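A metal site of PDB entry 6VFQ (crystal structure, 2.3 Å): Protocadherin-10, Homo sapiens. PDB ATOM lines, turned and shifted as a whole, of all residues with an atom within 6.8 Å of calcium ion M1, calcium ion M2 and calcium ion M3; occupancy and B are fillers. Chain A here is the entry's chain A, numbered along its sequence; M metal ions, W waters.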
ATOM      1  N   GLU A 116     -20.209 -13.198  16.367  1.00  0.00           N
ATOM      2  CA  GLU A 116     -20.395 -14.596  16.019  1.00  0.00           C
ATOM      3  C   GLU A 116     -20.067 -15.534  17.164  1.00  0.00           C
ATOM      4  O   GLU A 116     -20.420 -16.711  17.118  1.00  0.00           O
ATOM      5  CB  GLU A 116     -19.565 -14.961  14.784  1.00  0.00           C
ATOM      6  CG  GLU A 116     -18.081 -15.140  15.035  1.00  0.00           C
ATOM      7  CD  GLU A 116     -17.291 -15.528  13.777  1.00  0.00           C
ATOM      8  OE1 GLU A 116     -17.740 -16.405  13.012  1.00  0.00           O
ATOM      9  OE2 GLU A 116     -16.214 -14.943  13.580  1.00  0.00           O
ATOM     10  N   LEU A 172     -24.044 -18.320  15.424  1.00  0.00           N
ATOM     11  CA  LEU A 172     -23.794 -17.700  14.136  1.00  0.00           C
ATOM     12  C   LEU A 172     -22.353 -17.983  13.703  1.00  0.00           C
ATOM     13  O   LEU A 172     -21.473 -18.272  14.514  1.00  0.00           O
ATOM     14  CB  LEU A 172     -24.036 -16.196  14.202  1.00  0.00           C
ATOM     15  CG  LEU A 172     -25.347 -15.673  14.757  1.00  0.00           C
ATOM     16  CD1 LEU A 172     -25.100 -14.335  15.352  1.00  0.00           C
ATOM     17  CD2 LEU A 172     -26.361 -15.571  13.647  1.00  0.00           C
ATOM     18  N   ASP A 173     -22.104 -17.849  12.399  1.00  0.00           N
ATOM     19  CA  ASP A 173     -20.782 -18.079  11.821  1.00  0.00           C
ATOM     20  C   ASP A 173     -20.581 -17.042  10.740  1.00  0.00           C
ATOM     21  O   ASP A 173     -21.119 -17.185   9.627  1.00  0.00           O
ATOM     22  CB  ASP A 173     -20.657 -19.491  11.257  1.00  0.00           C
ATOM     23  CG  ASP A 173     -19.266 -19.802  10.664  1.00  0.00           C
ATOM     24  OD1 ASP A 173     -18.271 -19.069  10.927  1.00  0.00           O
ATOM     25  OD2 ASP A 173     -19.179 -20.813   9.921  1.00  0.00           O
ATOM     26  N   ARG A 174     -19.797 -16.005  11.042  1.00  0.00           N
ATOM     27  CA  ARG A 174     -19.615 -14.924  10.071  1.00  0.00           C
ATOM     28  C   ARG A 174     -19.010 -15.451   8.783  1.00  0.00           C
ATOM     29  O   ARG A 174     -19.328 -14.958   7.691  1.00  0.00           O
ATOM     30  CB  ARG A 174     -18.716 -13.848  10.645  1.00  0.00           C
ATOM     31  CG  ARG A 174     -18.580 -12.647   9.762  1.00  0.00           C
ATOM     32  CD  ARG A 174     -17.341 -11.844  10.131  1.00  0.00           C
ATOM     33  NE  ARG A 174     -16.156 -12.595   9.697  1.00  0.00           N
ATOM     34  CZ  ARG A 174     -15.755 -12.659   8.434  1.00  0.00           C
ATOM     35  NH1 ARG A 174     -16.409 -11.996   7.486  1.00  0.00           N
ATOM     36  NH2 ARG A 174     -14.698 -13.387   8.103  1.00  0.00           N
ATOM     37  N   GLU A 175     -18.098 -16.425   8.912  1.00  0.00           N
ATOM     38  CA  GLU A 175     -17.421 -16.989   7.760  1.00  0.00           C
ATOM     39  C   GLU A 175     -18.375 -17.749   6.851  1.00  0.00           C
ATOM     40  O   GLU A 175     -18.034 -18.034   5.703  1.00  0.00           O
ATOM     41  CB  GLU A 175     -16.288 -17.923   8.241  1.00  0.00           C
ATOM     42  CG  GLU A 175     -15.010 -17.202   8.714  1.00  0.00           C
ATOM     43  CD  GLU A 175     -15.092 -16.512  10.077  1.00  0.00           C
ATOM     44  OE1 GLU A 175     -14.802 -15.300  10.131  1.00  0.00           O
ATOM     45  OE2 GLU A 175     -15.385 -17.169  11.100  1.00  0.00           O
ATOM     46  N   GLN A 176     -19.569 -18.080   7.357  1.00  0.00           N
ATOM     47  CA  GLN A 176     -20.605 -18.738   6.565  1.00  0.00           C
ATOM     48  C   GLN A 176     -21.647 -17.770   6.040  1.00  0.00           C
ATOM     49  O   GLN A 176     -22.135 -17.930   4.920  1.00  0.00           O
ATOM     50  CB  GLN A 176     -21.306 -19.802   7.392  1.00  0.00           C
ATOM     51  CG  GLN A 176     -22.376 -20.557   6.631  1.00  0.00           C
ATOM     52  CD  GLN A 176     -22.599 -21.952   7.191  1.00  0.00           C
ATOM     53  OE1 GLN A 176     -21.869 -22.399   8.087  1.00  0.00           O
ATOM     54  NE2 GLN A 176     -23.584 -22.645   6.642  1.00  0.00           N
ATOM     55  N   LEU A 224     -20.494  -9.914  13.609  1.00  0.00           N
ATOM     56  CA  LEU A 224     -19.156  -9.377  13.827  1.00  0.00           C
ATOM     57  C   LEU A 224     -18.145 -10.505  13.988  1.00  0.00           C
ATOM     58  O   LEU A 224     -18.411 -11.523  14.642  1.00  0.00           O
ATOM     59  CB  LEU A 224     -19.142  -8.490  15.072  1.00  0.00           C
ATOM     60  CG  LEU A 224     -19.544  -7.044  14.830  1.00  0.00           C
ATOM     61  CD1 LEU A 224     -20.852  -6.939  14.106  1.00  0.00           C
ATOM     62  CD2 LEU A 224     -19.614  -6.328  16.181  1.00  0.00           C
ATOM     63  N   ASP A 225     -16.961 -10.309  13.410  1.00  0.00           N
ATOM     64  CA  ASP A 225     -15.946 -11.338  13.404  1.00  0.00           C
ATOM     65  C   ASP A 225     -15.335 -11.572  14.783  1.00  0.00           C
ATOM     66  O   ASP A 225     -15.084 -10.637  15.546  1.00  0.00           O
ATOM     67  CB  ASP A 225     -14.829 -10.960  12.436  1.00  0.00           C
ATOM     68  CG  ASP A 225     -13.831 -12.090  12.223  1.00  0.00           C
ATOM     69  OD1 ASP A 225     -14.253 -13.237  11.954  1.00  0.00           O
ATOM     70  OD2 ASP A 225     -12.624 -11.820  12.351  1.00  0.00           O
ATOM     71  N   SER A 226     -15.163 -12.839  15.113  1.00  0.00           N
ATOM     72  CA  SER A 226     -14.246 -13.275  16.157  1.00  0.00           C
ATOM     73  C   SER A 226     -13.087 -14.033  15.529  1.00  0.00           C
ATOM     74  O   SER A 226     -13.179 -14.539  14.405  1.00  0.00           O
ATOM     75  CB  SER A 226     -14.945 -14.169  17.176  1.00  0.00           C
ATOM     76  OG  SER A 226     -15.083 -15.481  16.658  1.00  0.00           O
ATOM     77  N   ASN A 227     -11.971 -14.113  16.279  1.00  0.00           N
ATOM     78  CA  ASN A 227     -10.778 -14.806  15.787  1.00  0.00           C
ATOM     79  C   ASN A 227     -10.877 -16.284  16.136  1.00  0.00           C
ATOM     80  O   ASN A 227     -10.217 -16.795  17.031  1.00  0.00           O
ATOM     81  CB  ASN A 227      -9.507 -14.180  16.368  1.00  0.00           C
ATOM     82  CG  ASN A 227      -8.236 -14.625  15.610  1.00  0.00           C
ATOM     83  OD1 ASN A 227      -8.309 -15.135  14.502  1.00  0.00           O
ATOM     84  ND2 ASN A 227      -7.079 -14.426  16.213  1.00  0.00           N
ATOM     85  N   ASP A 228     -11.760 -16.971  15.400  1.00  0.00           N
ATOM     86  CA  ASP A 228     -12.099 -18.360  15.677  1.00  0.00           C
ATOM     87  C   ASP A 228     -11.571 -19.331  14.627  1.00  0.00           C
ATOM     88  O   ASP A 228     -11.864 -20.530  14.701  1.00  0.00           O
ATOM     89  CB  ASP A 228     -13.624 -18.496  15.847  1.00  0.00           C
ATOM     90  CG  ASP A 228     -14.424 -18.038  14.624  1.00  0.00           C
ATOM     91  OD1 ASP A 228     -13.933 -17.258  13.776  1.00  0.00           O
ATOM     92  OD2 ASP A 228     -15.610 -18.452  14.519  1.00  0.00           O
ATOM     93  N   ASN A 229     -10.787 -18.856  13.650  1.00  0.00           N
ATOM     94  CA  ASN A 229     -10.116 -19.733  12.708  1.00  0.00           C
ATOM     95  C   ASN A 229      -8.612 -19.588  12.863  1.00  0.00           C
ATOM     96  O   ASN A 229      -8.087 -18.468  12.936  1.00  0.00           O
ATOM     97  CB  ASN A 229     -10.485 -19.421  11.268  1.00  0.00           C
ATOM     98  CG  ASN A 229     -11.873 -19.868  10.938  1.00  0.00           C
ATOM     99  OD1 ASN A 229     -12.109 -21.037  10.630  1.00  0.00           O
ATOM    100  ND2 ASN A 229     -12.838 -18.927  11.026  1.00  0.00           N
ATOM    101  N   VAL A 230      -7.936 -20.739  12.885  1.00  0.00           N
ATOM    102  CA  VAL A 230      -6.486 -20.831  13.010  1.00  0.00           C
ATOM    103  C   VAL A 230      -5.922 -20.931  11.605  1.00  0.00           C
ATOM    104  O   VAL A 230      -6.498 -21.634  10.777  1.00  0.00           O
ATOM    105  CB  VAL A 230      -6.080 -22.047  13.853  1.00  0.00           C
ATOM    106  CG1 VAL A 230      -4.547 -22.232  13.855  1.00  0.00           C
ATOM    107  CG2 VAL A 230      -6.671 -21.894  15.265  1.00  0.00           C
ATOM    108  N   PRO A 231      -4.809 -20.262  11.295  1.00  0.00           N
ATOM    109  CA  PRO A 231      -4.195 -20.434   9.978  1.00  0.00           C
ATOM    110  C   PRO A 231      -3.909 -21.908   9.704  1.00  0.00           C
ATOM    111  O   PRO A 231      -3.607 -22.689  10.600  1.00  0.00           O
ATOM    112  CB  PRO A 231      -2.908 -19.619  10.072  1.00  0.00           C
ATOM    113  CG  PRO A 231      -3.215 -18.573  11.100  1.00  0.00           C
ATOM    114  CD  PRO A 231      -4.093 -19.252  12.106  1.00  0.00           C
ATOM    115  N   ASP A 259      -6.456 -18.293   6.306  1.00  0.00           N
ATOM    116  CA  ASP A 259      -7.175 -17.873   7.510  1.00  0.00           C
ATOM    117  C   ASP A 259      -8.379 -17.063   7.050  1.00  0.00           C
ATOM    118  O   ASP A 259      -8.226 -15.926   6.606  1.00  0.00           O
ATOM    119  CB  ASP A 259      -6.260 -17.054   8.418  1.00  0.00           C
ATOM    120  CG  ASP A 259      -6.839 -16.857   9.823  1.00  0.00           C
ATOM    121  OD1 ASP A 259      -8.054 -16.579   9.993  1.00  0.00           O
ATOM    122  OD2 ASP A 259      -6.050 -16.954  10.794  1.00  0.00           O
ATOM    123  N   PRO A 260      -9.588 -17.614   7.124  1.00  0.00           N
ATOM    124  CA  PRO A 260     -10.765 -16.897   6.607  1.00  0.00           C
ATOM    125  C   PRO A 260     -11.299 -15.769   7.494  1.00  0.00           C
ATOM    126  O   PRO A 260     -12.264 -15.114   7.089  1.00  0.00           O
ATOM    127  CB  PRO A 260     -11.804 -17.999   6.474  1.00  0.00           C
ATOM    128  CG  PRO A 260     -11.404 -19.007   7.522  1.00  0.00           C
ATOM    129  CD  PRO A 260      -9.918 -18.975   7.583  1.00  0.00           C
ATOM    130  N   ASP A 261     -10.720 -15.493   8.669  1.00  0.00           N
ATOM    131  CA  ASP A 261     -11.243 -14.431   9.511  1.00  0.00           C
ATOM    132  C   ASP A 261     -11.092 -13.085   8.824  1.00  0.00           C
ATOM    133  O   ASP A 261     -10.547 -12.980   7.728  1.00  0.00           O
ATOM    134  CB  ASP A 261     -10.555 -14.433  10.873  1.00  0.00           C
ATOM    135  CG  ASP A 261     -10.935 -15.630  11.709  1.00  0.00           C
ATOM    136  OD1 ASP A 261     -12.109 -16.029  11.659  1.00  0.00           O
ATOM    137  OD2 ASP A 261     -10.049 -16.192  12.398  1.00  0.00           O
ATOM    138  N   GLU A 262     -11.559 -12.036   9.489  1.00  0.00           N
ATOM    139  CA  GLU A 262     -11.603 -10.684   8.947  1.00  0.00           C
ATOM    140  C   GLU A 262     -10.560  -9.796   9.637  1.00  0.00           C
ATOM    141  O   GLU A 262     -10.199 -10.029  10.785  1.00  0.00           O
ATOM    142  CB  GLU A 262     -13.013 -10.112   9.147  1.00  0.00           C
ATOM    143  CG  GLU A 262     -13.215  -8.677   8.772  1.00  0.00           C
ATOM    144  CD  GLU A 262     -14.651  -8.228   9.056  1.00  0.00           C
ATOM    145  OE1 GLU A 262     -15.497  -8.351   8.152  1.00  0.00           O
ATOM    146  OE2 GLU A 262     -14.928  -7.781  10.196  1.00  0.00           O
ATOM    147  N   GLN A 264      -7.284  -7.983  11.080  1.00  0.00           N
ATOM    148  CA  GLN A 264      -6.087  -8.547  11.694  1.00  0.00           C
ATOM    149  C   GLN A 264      -6.290 -10.015  12.057  1.00  0.00           C
ATOM    150  O   GLN A 264      -5.356 -10.815  11.956  1.00  0.00           O
ATOM    151  CB  GLN A 264      -5.715  -7.723  12.932  1.00  0.00           C
ATOM    152  CG  GLN A 264      -5.365  -6.255  12.627  1.00  0.00           C
ATOM    153  CD  GLN A 264      -4.330  -6.107  11.516  1.00  0.00           C
ATOM    154  OE1 GLN A 264      -3.112  -6.266  11.731  1.00  0.00           O
ATOM    155  NE2 GLN A 264      -4.813  -5.847  10.300  1.00  0.00           N
ATOM    156  N   ASN A 265      -7.517 -10.397  12.461  1.00  0.00           N
ATOM    157  CA  ASN A 265      -7.810 -11.792  12.759  1.00  0.00           C
ATOM    158  C   ASN A 265      -7.451 -12.696  11.599  1.00  0.00           C
ATOM    159  O   ASN A 265      -7.176 -13.883  11.800  1.00  0.00           O
ATOM    160  CB  ASN A 265      -9.292 -11.990  13.091  1.00  0.00           C
ATOM    161  CG  ASN A 265      -9.713 -11.217  14.298  1.00  0.00           C
ATOM    162  OD1 ASN A 265      -8.889 -10.879  15.136  1.00  0.00           O
ATOM    163  ND2 ASN A 265     -11.005 -10.918  14.392  1.00  0.00           N
ATOM    164  N   GLY A 266      -7.489 -12.157  10.386  1.00  0.00           N
ATOM    165  CA  GLY A 266      -7.274 -12.972   9.213  1.00  0.00           C
ATOM    166  C   GLY A 266      -5.963 -12.710   8.494  1.00  0.00           C
ATOM    167  O   GLY A 266      -5.693 -13.346   7.476  1.00  0.00           O
ATOM    168  N   GLU A 267      -5.162 -11.771   9.003  1.00  0.00           N
ATOM    169  CA  GLU A 267      -3.854 -11.470   8.427  1.00  0.00           C
ATOM    170  C   GLU A 267      -2.792 -12.354   9.061  1.00  0.00           C
ATOM    171  O   GLU A 267      -2.666 -12.397  10.294  1.00  0.00           O
ATOM    172  CB  GLU A 267      -3.491  -9.990   8.637  1.00  0.00           C
ATOM    173  CG  GLU A 267      -4.195  -9.012   7.722  1.00  0.00           C
ATOM    174  CD  GLU A 267      -3.856  -9.222   6.248  1.00  0.00           C
ATOM    175  OE1 GLU A 267      -2.672  -9.481   5.917  1.00  0.00           O
ATOM    176  OE2 GLU A 267      -4.791  -9.143   5.422  1.00  0.00           O
ATOM    177  N   VAL A 268      -2.020 -13.055   8.217  1.00  0.00           N
ATOM    178  CA  VAL A 268      -1.087 -14.082   8.656  1.00  0.00           C
ATOM    179  C   VAL A 268       0.350 -13.602   8.431  1.00  0.00           C
ATOM    180  O   VAL A 268       0.694 -13.089   7.360  1.00  0.00           O
ATOM    181  CB  VAL A 268      -1.328 -15.400   7.894  1.00  0.00           C
ATOM    182  CG1 VAL A 268      -0.350 -16.450   8.349  1.00  0.00           C
ATOM    183  CG2 VAL A 268      -2.718 -15.860   8.108  1.00  0.00           C
ATOM    184  N   ASP A 315      -1.870 -15.615  12.974  1.00  0.00           N
ATOM    185  CA  ASP A 315      -2.544 -14.404  12.528  1.00  0.00           C
ATOM    186  C   ASP A 315      -2.221 -13.271  13.505  1.00  0.00           C
ATOM    187  O   ASP A 315      -1.556 -13.474  14.520  1.00  0.00           O
ATOM    188  CB  ASP A 315      -4.038 -14.640  12.330  1.00  0.00           C
ATOM    189  CG  ASP A 315      -4.810 -14.949  13.624  1.00  0.00           C
ATOM    190  OD1 ASP A 315      -4.691 -14.200  14.620  1.00  0.00           O
ATOM    191  OD2 ASP A 315      -5.559 -15.954  13.628  1.00  0.00           O
ATOM    192  N   LEU A 316      -2.653 -12.066  13.154  1.00  0.00           N
ATOM    193  CA  LEU A 316      -2.350 -10.876  13.921  1.00  0.00           C
ATOM    194  C   LEU A 316      -3.470 -10.466  14.889  1.00  0.00           C
ATOM    195  O   LEU A 316      -3.450  -9.348  15.425  1.00  0.00           O
ATOM    196  CB  LEU A 316      -2.029  -9.737  12.967  1.00  0.00           C
ATOM    197  CG  LEU A 316      -0.741  -9.875  12.155  1.00  0.00           C
ATOM    198  CD1 LEU A 316      -0.655  -8.819  11.079  1.00  0.00           C
ATOM    199  CD2 LEU A 316       0.467  -9.764  13.017  1.00  0.00           C
ATOM    200  N   GLY A 317      -4.442 -11.339  15.150  1.00  0.00           N
ATOM    201  CA  GLY A 317      -5.544 -10.997  16.039  1.00  0.00           C
ATOM    202  C   GLY A 317      -5.260 -11.354  17.496  1.00  0.00           C
ATOM    203  O   GLY A 317      -4.241 -11.965  17.825  1.00  0.00           O
ATOM    204  N   ALA A 320      -4.434 -15.251  19.180  1.00  0.00           N
ATOM    205  CA  ALA A 320      -4.038 -16.034  18.016  1.00  0.00           C
ATOM    206  C   ALA A 320      -3.388 -17.339  18.436  1.00  0.00           C
ATOM    207  O   ALA A 320      -2.676 -17.420  19.438  1.00  0.00           O
ATOM    208  CB  ALA A 320      -3.084 -15.225  17.143  1.00  0.00           C
HETATM  209 CA    CA M   1     -14.224 -15.414  12.432  1.00  0.00          CA
HETATM  210 CA    CA M   2     -16.765 -18.492  12.556  1.00  0.00          CA
HETATM  211 CA    CA M   3      -7.644 -16.185  12.481  1.00  0.00          CA
HETATM  212  O   HOH W   1     -18.418 -19.920  13.390  1.00  0.00           O
HETATM  213  O   HOH W   2     -15.249 -20.248  11.998  1.00  0.00           O
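The guanidinium group of Arg 174 sits close to the side-chain carboxylate of Asp 225 (3.0 Å).
The backbone NH of Glu 116 is in hydrogen-bond range of the backbone carbonyl oxygen of Leu 224, 3.0 Å away.
The side-chain amide nitrogen (ND2) of Asn 229 sits close to the side-chain carboxylate (OE2) of Glu 175.
The side-chain carboxylate (OD2) of Asp 225 sits at hydrogen-bond distance from the backbone NH (N) of Glu 262, 3.1 Å away.
ND2 of Asn 229 lies close to OD1 of Asp 228 (3.4 Å).
The side-chain carboxylate (OE1) of Glu 175 sits close to the guanidinium group (NH2) of Arg 174.
The side-chain carboxylate (OD2) of Asp 225 sits at hydrogen-bond distance from the side-chain amide nitrogen (ND2) of Asn 265, at 2.8 Å.
The side-chain carboxylate (OD1) of Asp 315 sits at hydrogen-bond distance from the backbone NH (N) of Gly 317.
Of the 27 residues printed, 4 come within 4 Å of calcium ion M2.
Calcium ion M2 is bound by the side-chain carboxylate of Asp 228, the side-chain carboxylate of Asp 173, water W1, the side-chain carboxylate of Glu 116, water W2 and the side-chain carboxylate of Glu 175.
Calcium ion M2 has six donor atoms within binding distance.
The side-chain carboxylate (OD1) of Asp 225 binds calcium ion M1.
Calcium ion M1 is bound by OD1 of Asp 228, at 2.3 Å.
Calcium ion M1 is bound by OD1 of Asp 261 (2.3 Å).
Calcium ion M1 is bound by OE2 of Glu 116 (2.3 Å).
Calcium ion M1 is bound by OE1 of Glu 175 (2.4 Å).
The backbone carbonyl oxygen (O) of Ser 226 is bound to calcium ion M1, 2.4 Å away.
OE2 of Glu 175 binds calcium ion M1 (2.5 Å).
Calcium ion M3 is bound by O of Asn 229 (2.4 Å).
OD1 of Asn 227 binds calcium ion M3, 2.4 Å away.
Calcium ion M3 is bound by the side-chain carboxylate (OD2) of Asp 315 (2.4 Å).
The side-chain carboxylate (OD2) of Asp 261 binds calcium ion M3, 2.4 Å away.
The backbone carbonyl oxygen (O) of Asn 265 binds calcium ion M3 (2.4 Å).
The side-chain carboxylate (OD2) of Asp 259 binds calcium ion M3, 2.4 Å away.
Calcium ion M3 is bound by OD1 of Asp 259, at 2.6 Å.
Six residues have an atom within 4 Å of calcium ion M3: Asn 227, Asn 229, Asp 259, Asp 261, Asn 265 and Asp 315.
The nearest printed residue that does not touch calcium ion M3 is Gly 266 (4.5 Å).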
